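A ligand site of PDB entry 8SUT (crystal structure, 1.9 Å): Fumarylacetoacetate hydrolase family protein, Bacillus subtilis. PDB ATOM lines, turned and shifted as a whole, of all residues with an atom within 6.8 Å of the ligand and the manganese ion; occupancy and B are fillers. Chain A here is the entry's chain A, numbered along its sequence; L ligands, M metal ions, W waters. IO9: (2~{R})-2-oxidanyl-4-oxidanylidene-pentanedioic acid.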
ATOM      1  N   CYS A  99     -18.108  11.129   4.354  1.00  0.00           N
ATOM      2  CA  CYS A  99     -17.792  12.320   3.587  1.00  0.00           C
ATOM      3  C   CYS A  99     -16.293  12.493   3.426  1.00  0.00           C
ATOM      4  O   CYS A  99     -15.525  12.298   4.369  1.00  0.00           O
ATOM      5  CB  CYS A  99     -18.385  13.557   4.239  1.00  0.00           C
ATOM      6  SG  CYS A  99     -20.164  13.518   4.420  1.00  0.00           S
ATOM      7  N   ILE A 100     -15.893  12.845   2.195  1.00  0.00           N
ATOM      8  CA  ILE A 100     -14.513  13.173   1.888  1.00  0.00           C
ATOM      9  C   ILE A 100     -14.373  14.693   1.902  1.00  0.00           C
ATOM     10  O   ILE A 100     -15.174  15.404   1.300  1.00  0.00           O
ATOM     11  CB  ILE A 100     -14.063  12.549   0.550  1.00  0.00           C
ATOM     12  CG1 ILE A 100     -14.528  11.087   0.424  1.00  0.00           C
ATOM     13  CG2 ILE A 100     -12.542  12.678   0.355  1.00  0.00           C
ATOM     14  CD1 ILE A 100     -14.020  10.116   1.574  1.00  0.00           C
ATOM     15  N   GLY A 101     -13.355  15.178   2.620  1.00  0.00           N
ATOM     16  CA  GLY A 101     -12.984  16.579   2.588  1.00  0.00           C
ATOM     17  C   GLY A 101     -11.875  16.879   1.581  1.00  0.00           C
ATOM     18  O   GLY A 101     -10.955  16.072   1.434  1.00  0.00           O
ATOM     19  N   LYS A 102     -11.964  18.034   0.922  1.00  0.00           N
ATOM     20  CA  LYS A 102     -10.895  18.532   0.065  1.00  0.00           C
ATOM     21  C   LYS A 102     -10.418  17.483  -0.932  1.00  0.00           C
ATOM     22  O   LYS A 102      -9.267  17.050  -0.899  1.00  0.00           O
ATOM     23  CB  LYS A 102      -9.709  19.010   0.919  1.00  0.00           C
ATOM     24  CG  LYS A 102     -10.072  20.108   1.932  1.00  0.00           C
ATOM     25  CD  LYS A 102      -8.875  20.573   2.768  1.00  0.00           C
ATOM     26  CE  LYS A 102      -8.897  22.055   3.086  1.00  0.00           C
ATOM     27  NZ  LYS A 102     -10.197  22.488   3.685  1.00  0.00           N
ATOM     28  N   ASN A 103     -11.316  17.084  -1.840  1.00  0.00           N
ATOM     29  CA  ASN A 103     -10.987  16.110  -2.867  1.00  0.00           C
ATOM     30  C   ASN A 103     -10.926  16.741  -4.252  1.00  0.00           C
ATOM     31  O   ASN A 103     -10.793  16.038  -5.254  1.00  0.00           O
ATOM     32  CB  ASN A 103     -12.000  14.957  -2.818  1.00  0.00           C
ATOM     33  CG  ASN A 103     -11.502  13.690  -3.500  1.00  0.00           C
ATOM     34  OD1 ASN A 103     -10.310  13.426  -3.501  1.00  0.00           O
ATOM     35  ND2 ASN A 103     -12.397  12.891  -4.076  1.00  0.00           N
ATOM     36  N   TYR A 104     -11.061  18.079  -4.306  1.00  0.00           N
ATOM     37  CA  TYR A 104     -10.822  18.850  -5.523  1.00  0.00           C
ATOM     38  C   TYR A 104      -9.773  19.913  -5.177  1.00  0.00           C
ATOM     39  O   TYR A 104      -9.905  20.594  -4.164  1.00  0.00           O
ATOM     40  CB  TYR A 104     -12.076  19.544  -6.053  1.00  0.00           C
ATOM     41  CG  TYR A 104     -13.105  18.622  -6.663  1.00  0.00           C
ATOM     42  CD1 TYR A 104     -13.916  17.827  -5.855  1.00  0.00           C
ATOM     43  CD2 TYR A 104     -13.308  18.586  -8.032  1.00  0.00           C
ATOM     44  CE1 TYR A 104     -14.880  16.985  -6.399  1.00  0.00           C
ATOM     45  CE2 TYR A 104     -14.288  17.764  -8.588  1.00  0.00           C
ATOM     46  CZ  TYR A 104     -15.071  16.962  -7.761  1.00  0.00           C
ATOM     47  OH  TYR A 104     -16.046  16.120  -8.260  1.00  0.00           O
ATOM     48  N   HIS A 107     -10.946  23.529  -4.434  1.00  0.00           N
ATOM     49  CA  HIS A 107     -11.704  23.641  -3.192  1.00  0.00           C
ATOM     50  C   HIS A 107     -10.749  23.779  -2.002  1.00  0.00           C
ATOM     51  O   HIS A 107     -10.967  24.626  -1.129  1.00  0.00           O
ATOM     52  CB  HIS A 107     -12.620  22.437  -2.941  1.00  0.00           C
ATOM     53  CG  HIS A 107     -13.378  22.589  -1.667  1.00  0.00           C
ATOM     54  ND1 HIS A 107     -14.222  23.655  -1.483  1.00  0.00           N
ATOM     55  CD2 HIS A 107     -13.379  21.898  -0.504  1.00  0.00           C
ATOM     56  CE1 HIS A 107     -14.733  23.597  -0.246  1.00  0.00           C
ATOM     57  NE2 HIS A 107     -14.251  22.532   0.355  1.00  0.00           N
ATOM     58  N   ALA A 108      -9.716  22.915  -1.962  1.00  0.00           N
ATOM     59  CA  ALA A 108      -8.679  22.949  -0.949  1.00  0.00           C
ATOM     60  C   ALA A 108      -7.976  24.310  -0.884  1.00  0.00           C
ATOM     61  O   ALA A 108      -7.712  24.830   0.211  1.00  0.00           O
ATOM     62  CB  ALA A 108      -7.667  21.837  -1.211  1.00  0.00           C
ATOM     63  N   MET A 111     -10.118  27.261   0.495  1.00  0.00           N
ATOM     64  CA  MET A 111     -10.345  27.130   1.937  1.00  0.00           C
ATOM     65  C   MET A 111      -9.067  27.395   2.748  1.00  0.00           C
ATOM     66  O   MET A 111      -9.085  27.273   3.972  1.00  0.00           O
ATOM     67  CB  MET A 111     -10.893  25.705   2.270  1.00  0.00           C
ATOM     68  CG  MET A 111     -12.286  25.418   1.682  1.00  0.00           C
ATOM     69  SD  MET A 111     -13.647  26.473   2.291  1.00  0.00           S
ATOM     70  CE  MET A 111     -13.616  26.087   4.078  1.00  0.00           C
ATOM     71  N   MET A 122      -9.170  12.866   3.691  1.00  0.00           N
ATOM     72  CA  MET A 122      -9.677  13.325   4.975  1.00  0.00           C
ATOM     73  C   MET A 122     -11.134  12.857   5.004  1.00  0.00           C
ATOM     74  O   MET A 122     -11.917  13.261   4.149  1.00  0.00           O
ATOM     75  CB  MET A 122      -9.480  14.841   5.090  1.00  0.00           C
ATOM     76  CG  MET A 122     -10.515  15.575   5.897  1.00  0.00           C
ATOM     77  SD  MET A 122     -10.181  17.368   5.969  1.00  0.00           S
ATOM     78  CE  MET A 122      -8.568  17.401   6.642  1.00  0.00           C
ATOM     79  N   PHE A 124     -14.712  12.166   7.200  1.00  0.00           N
ATOM     80  CA  PHE A 124     -15.571  12.419   8.345  1.00  0.00           C
ATOM     81  C   PHE A 124     -16.983  11.946   7.999  1.00  0.00           C
ATOM     82  O   PHE A 124     -17.209  11.375   6.935  1.00  0.00           O
ATOM     83  CB  PHE A 124     -15.492  13.912   8.717  1.00  0.00           C
ATOM     84  CG  PHE A 124     -15.960  14.766   7.586  1.00  0.00           C
ATOM     85  CD1 PHE A 124     -15.087  15.147   6.572  1.00  0.00           C
ATOM     86  CD2 PHE A 124     -17.285  15.143   7.486  1.00  0.00           C
ATOM     87  CE1 PHE A 124     -15.524  15.920   5.512  1.00  0.00           C
ATOM     88  CE2 PHE A 124     -17.719  15.908   6.411  1.00  0.00           C
ATOM     89  CZ  PHE A 124     -16.835  16.289   5.432  1.00  0.00           C
ATOM     90  N   GLU A 151     -22.608  22.625  -0.367  1.00  0.00           N
ATOM     91  CA  GLU A 151     -21.584  21.836  -1.057  1.00  0.00           C
ATOM     92  C   GLU A 151     -22.226  20.778  -1.957  1.00  0.00           C
ATOM     93  O   GLU A 151     -22.709  19.755  -1.467  1.00  0.00           O
ATOM     94  CB  GLU A 151     -20.682  21.133  -0.030  1.00  0.00           C
ATOM     95  CG  GLU A 151     -19.935  22.035   0.937  1.00  0.00           C
ATOM     96  CD  GLU A 151     -18.895  21.315   1.777  1.00  0.00           C
ATOM     97  OE1 GLU A 151     -18.812  20.083   1.615  1.00  0.00           O
ATOM     98  OE2 GLU A 151     -18.155  21.955   2.549  1.00  0.00           O
ATOM     99  N   GLY A 152     -22.255  21.001  -3.265  1.00  0.00           N
ATOM    100  CA  GLY A 152     -22.752  19.996  -4.179  1.00  0.00           C
ATOM    101  C   GLY A 152     -21.739  18.873  -4.344  1.00  0.00           C
ATOM    102  O   GLY A 152     -20.556  19.156  -4.544  1.00  0.00           O
ATOM    103  N   GLU A 153     -22.182  17.621  -4.234  1.00  0.00           N
ATOM    104  CA  GLU A 153     -21.290  16.473  -4.370  1.00  0.00           C
ATOM    105  C   GLU A 153     -21.933  15.273  -5.062  1.00  0.00           C
ATOM    106  O   GLU A 153     -23.157  15.074  -5.000  1.00  0.00           O
ATOM    107  CB  GLU A 153     -20.786  15.976  -3.004  1.00  0.00           C
ATOM    108  CG  GLU A 153     -20.445  17.101  -2.087  1.00  0.00           C
ATOM    109  CD  GLU A 153     -19.650  16.713  -0.861  1.00  0.00           C
ATOM    110  OE1 GLU A 153     -19.183  15.548  -0.732  1.00  0.00           O
ATOM    111  OE2 GLU A 153     -19.506  17.604  -0.014  1.00  0.00           O
ATOM    112  N   ASP A 182     -23.905  18.693   0.889  1.00  0.00           N
ATOM    113  CA  ASP A 182     -23.270  18.547   2.193  1.00  0.00           C
ATOM    114  C   ASP A 182     -23.259  19.893   2.916  1.00  0.00           C
ATOM    115  O   ASP A 182     -22.220  20.530   3.059  1.00  0.00           O
ATOM    116  CB  ASP A 182     -21.846  17.982   2.003  1.00  0.00           C
ATOM    117  CG  ASP A 182     -21.016  17.839   3.280  1.00  0.00           C
ATOM    118  OD1 ASP A 182     -21.588  17.900   4.397  1.00  0.00           O
ATOM    119  OD2 ASP A 182     -19.812  17.672   3.160  1.00  0.00           O
ATOM    120  N   THR A 184     -23.105  22.648   5.584  1.00  0.00           N
ATOM    121  CA  THR A 184     -22.129  22.749   6.653  1.00  0.00           C
ATOM    122  C   THR A 184     -22.247  24.076   7.408  1.00  0.00           C
ATOM    123  O   THR A 184     -22.414  25.129   6.796  1.00  0.00           O
ATOM    124  CB  THR A 184     -20.724  22.610   6.031  1.00  0.00           C
ATOM    125  OG1 THR A 184     -20.674  21.397   5.256  1.00  0.00           O
ATOM    126  CG2 THR A 184     -19.600  22.610   7.073  1.00  0.00           C
ATOM    127  N   ARG A 186     -19.953  26.438   9.087  1.00  0.00           N
ATOM    128  CA  ARG A 186     -18.505  26.614   9.029  1.00  0.00           C
ATOM    129  C   ARG A 186     -17.877  27.032  10.360  1.00  0.00           C
ATOM    130  O   ARG A 186     -16.733  26.659  10.661  1.00  0.00           O
ATOM    131  CB  ARG A 186     -18.137  27.699   8.003  1.00  0.00           C
ATOM    132  CG  ARG A 186     -18.536  27.358   6.559  1.00  0.00           C
ATOM    133  CD  ARG A 186     -17.569  26.387   5.953  1.00  0.00           C
ATOM    134  NE  ARG A 186     -17.980  26.017   4.607  1.00  0.00           N
ATOM    135  CZ  ARG A 186     -17.714  24.840   4.025  1.00  0.00           C
ATOM    136  NH1 ARG A 186     -16.983  23.916   4.627  1.00  0.00           N
ATOM    137  NH2 ARG A 186     -18.186  24.615   2.799  1.00  0.00           N
ATOM    138  N   GLN A 189     -17.702  23.887  12.503  1.00  0.00           N
ATOM    139  CA  GLN A 189     -16.538  23.130  12.082  1.00  0.00           C
ATOM    140  C   GLN A 189     -15.262  23.557  12.786  1.00  0.00           C
ATOM    141  O   GLN A 189     -14.478  22.712  13.238  1.00  0.00           O
ATOM    142  CB  GLN A 189     -16.274  23.287  10.586  1.00  0.00           C
ATOM    143  CG  GLN A 189     -16.987  22.367   9.679  1.00  0.00           C
ATOM    144  CD  GLN A 189     -16.418  22.532   8.285  1.00  0.00           C
ATOM    145  OE1 GLN A 189     -16.509  23.605   7.673  1.00  0.00           O
ATOM    146  NE2 GLN A 189     -15.814  21.494   7.749  1.00  0.00           N
ATOM    147  N   PHE A 195     -15.171  17.644  12.380  1.00  0.00           N
ATOM    148  CA  PHE A 195     -16.243  18.221  11.588  1.00  0.00           C
ATOM    149  C   PHE A 195     -17.649  17.740  11.904  1.00  0.00           C
ATOM    150  O   PHE A 195     -18.628  18.337  11.453  1.00  0.00           O
ATOM    151  CB  PHE A 195     -15.952  17.931  10.106  1.00  0.00           C
ATOM    152  CG  PHE A 195     -14.792  18.668   9.479  1.00  0.00           C
ATOM    153  CD1 PHE A 195     -14.115  19.669  10.191  1.00  0.00           C
ATOM    154  CD2 PHE A 195     -14.367  18.361   8.206  1.00  0.00           C
ATOM    155  CE1 PHE A 195     -13.052  20.355   9.602  1.00  0.00           C
ATOM    156  CE2 PHE A 195     -13.290  19.044   7.627  1.00  0.00           C
ATOM    157  CZ  PHE A 195     -12.647  20.035   8.333  1.00  0.00           C
ATOM    158  N   LYS A 199     -21.238  19.369  10.553  1.00  0.00           N
ATOM    159  CA  LYS A 199     -21.766  18.603   9.436  1.00  0.00           C
ATOM    160  C   LYS A 199     -23.088  17.892   9.723  1.00  0.00           C
ATOM    161  O   LYS A 199     -23.740  17.403   8.796  1.00  0.00           O
ATOM    162  CB  LYS A 199     -20.728  17.549   9.025  1.00  0.00           C
ATOM    163  CG  LYS A 199     -19.455  18.129   8.453  1.00  0.00           C
ATOM    164  CD  LYS A 199     -19.664  18.627   7.060  1.00  0.00           C
ATOM    165  CE  LYS A 199     -18.409  19.191   6.468  1.00  0.00           C
ATOM    166  NZ  LYS A 199     -18.604  19.505   5.046  1.00  0.00           N
ATOM    167  N   ALA A 266     -20.048  10.462   0.083  1.00  0.00           N
ATOM    168  CA  ALA A 266     -20.007  11.774  -0.547  1.00  0.00           C
ATOM    169  C   ALA A 266     -18.547  12.101  -0.876  1.00  0.00           C
ATOM    170  O   ALA A 266     -17.733  12.229   0.034  1.00  0.00           O
ATOM    171  CB  ALA A 266     -20.608  12.815   0.398  1.00  0.00           C
ATOM    172  N   THR A 267     -18.251  12.277  -2.169  1.00  0.00           N
ATOM    173  CA  THR A 267     -16.885  12.273  -2.662  1.00  0.00           C
ATOM    174  C   THR A 267     -16.189  13.637  -2.697  1.00  0.00           C
ATOM    175  O   THR A 267     -15.096  13.758  -3.244  1.00  0.00           O
ATOM    176  CB  THR A 267     -16.894  11.601  -4.070  1.00  0.00           C
ATOM    177  OG1 THR A 267     -17.721  12.360  -4.953  1.00  0.00           O
ATOM    178  CG2 THR A 267     -17.395  10.196  -4.007  1.00  0.00           C
ATOM    179  N   GLY A 268     -16.824  14.665  -2.122  1.00  0.00           N
ATOM    180  CA  GLY A 268     -16.199  15.974  -1.995  1.00  0.00           C
ATOM    181  C   GLY A 268     -16.770  16.963  -3.000  1.00  0.00           C
ATOM    182  O   GLY A 268     -17.216  16.591  -4.076  1.00  0.00           O
ATOM    183  N   THR A 269     -16.749  18.244  -2.594  1.00  0.00           N
ATOM    184  CA  THR A 269     -17.333  19.326  -3.381  1.00  0.00           C
ATOM    185  C   THR A 269     -16.246  20.053  -4.162  1.00  0.00           C
ATOM    186  O   THR A 269     -15.112  20.187  -3.695  1.00  0.00           O
ATOM    187  CB  THR A 269     -18.101  20.243  -2.415  1.00  0.00           C
ATOM    188  OG1 THR A 269     -19.001  21.048  -3.162  1.00  0.00           O
ATOM    189  CG2 THR A 269     -17.181  21.141  -1.560  1.00  0.00           C
ATOM    190  N   PRO A 270     -16.533  20.555  -5.385  1.00  0.00           N
ATOM    191  CA  PRO A 270     -15.597  21.442  -6.085  1.00  0.00           C
ATOM    192  C   PRO A 270     -15.472  22.806  -5.395  1.00  0.00           C
ATOM    193  O   PRO A 270     -16.143  23.076  -4.396  1.00  0.00           O
ATOM    194  CB  PRO A 270     -16.219  21.600  -7.484  1.00  0.00           C
ATOM    195  CG  PRO A 270     -17.345  20.650  -7.546  1.00  0.00           C
ATOM    196  CD  PRO A 270     -17.778  20.347  -6.142  1.00  0.00           C
ATOM    197  N   VAL A 273     -17.720  27.244  -2.996  1.00  0.00           N
ATOM    198  CA  VAL A 273     -18.525  27.283  -1.782  1.00  0.00           C
ATOM    199  C   VAL A 273     -18.586  28.732  -1.290  1.00  0.00           C
ATOM    200  O   VAL A 273     -17.735  29.558  -1.639  1.00  0.00           O
ATOM    201  CB  VAL A 273     -18.049  26.305  -0.671  1.00  0.00           C
ATOM    202  CG1 VAL A 273     -17.872  24.893  -1.232  1.00  0.00           C
ATOM    203  CG2 VAL A 273     -16.766  26.796   0.033  1.00  0.00           C
HETATM  204  C01 IO9 L   1     -13.724  21.873   4.033  1.00  0.00           C
HETATM  205  C02 IO9 L   1     -15.507  18.853   1.112  1.00  0.00           C
HETATM  206  C03 IO9 L   1     -14.968  21.064   3.637  1.00  0.00           C
HETATM  207  C04 IO9 L   1     -14.631  19.599   3.470  1.00  0.00           C
HETATM  208  C05 IO9 L   1     -15.719  18.918   2.647  1.00  0.00           C
HETATM  209  O01 IO9 L   1     -13.001  22.370   3.123  1.00  0.00           O
HETATM  210  O02 IO9 L   1     -13.422  22.021   5.249  1.00  0.00           O
HETATM  211  O03 IO9 L   1     -14.425  19.177   0.604  1.00  0.00           O
HETATM  212  O04 IO9 L   1     -16.393  18.453   0.317  1.00  0.00           O
HETATM  213  O05 IO9 L   1     -15.958  21.126   4.633  1.00  0.00           O
HETATM  214  O06 IO9 L   1     -16.684  18.461   3.211  1.00  0.00           O
HETATM  215 MN    MN M   1     -18.189  17.956   1.624  1.00  0.00          MN
HETATM  216  O   HOH W   1     -13.699  18.836  -1.823  1.00  0.00           O
HETATM  217  O   HOH W   2     -18.013  15.630   1.609  1.00  0.00           O
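The manganese ion is bound by OE2 of Glu 153 (2.1 Å), OE1 of Glu 151 (2.2 Å), O06 of the ligand (2.2 Å), OD2 of Asp 182 (2.3 Å), O04 of the ligand (2.3 Å) and water W2 (2.3 Å). The manganese ion has six donor atoms within binding distance.
N of Gly 268 is in hydrogen-bond range of OE1 of Glu 153 (2.9 Å). OE2 of Glu 151 is in salt-bridge range of NH2 of Arg 186. O of Asp 182 sits at hydrogen-bond distance from OG1 of Thr 184 (2.8 Å). The side-chain hydroxyl (OG1) of Thr 184 lies within hydrogen-bond range of the side-chain amino group (NZ) of Lys 199. O of Gly 152 lies within hydrogen-bond range of OG1 of Thr 269 (2.8 Å). The side-chain amide oxygen of Gln 189 is in hydrogen-bond range of the guanidinium group of Arg 186, at 3.1 Å. N of Ile 100 lies within hydrogen-bond range of O of Ala 266, 2.9 Å away. The backbone carbonyl oxygen (O) of Met 122 is in hydrogen-bond range of the backbone NH (N) of Gly 101 (2.8 Å).
Merely in contact with the manganese ion: Lys 199 and Ile 100. Five residues have an atom within 4 Å of the manganese ion: Ile 100, Glu 151, Glu 153, Asp 182 and Lys 199.
The backbone carbonyl oxygen (O) of Ile 100 sits close to an oxygen (O04) of the ligand (3.4 Å). CA of Gly 101 touches C04 of the ligand, 3.6 Å away. Met 111 touches the ligand. Phe 124 touches the ligand (CZ to O06, 3.1 Å). Phe 195 touches the ligand (CZ to O02, 3.7 Å). Gly 268 touches the ligand. 15 residues have an atom within 4 Å of the ligand: Ile 100, Gly 101, Lys 102, His 107, Met 111, Phe 124, Glu 151, Glu 153, Asp 182, Arg 186, Gln 189, Phe 195, Lys 199, Gly 268 and Thr 269.
Water W2 bridges OE1 of Glu 153 (2.6 Å) and O of Ile 100 (2.9 Å). Water W1 lies within hydrogen-bond range of an oxygen (O03) of the ligand (2.6 Å), the backbone carbonyl oxygen of Thr 269 (2.7 Å), the backbone NH of Asn 103 (3.0 Å) and the backbone NH of Lys 102 (3.3 Å).
The backbone NH (N) of Lys 102 lies within hydrogen-bond range of an oxygen (O03) of the ligand (2.7 Å). NZ of Lys 102 lies within salt-bridge range of O01 of the ligand, at 2.9 Å. O05 of the ligand lies within hydrogen-bond range of NZ of Lys 199 (3.1 Å). An oxygen (O04) of the ligand sits close to the backbone NH of Thr 269. The guanidinium group (NH1) of Arg 186 is in hydrogen-bond range of an oxygen (O05) of the ligand. NE2 of His 107 lies within hydrogen-bond range of O01 of the ligand (3.0 Å). The side-chain amide nitrogen of Gln 189 sits at hydrogen-bond distance from an oxygen (O05) of the ligand (3.1 Å).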
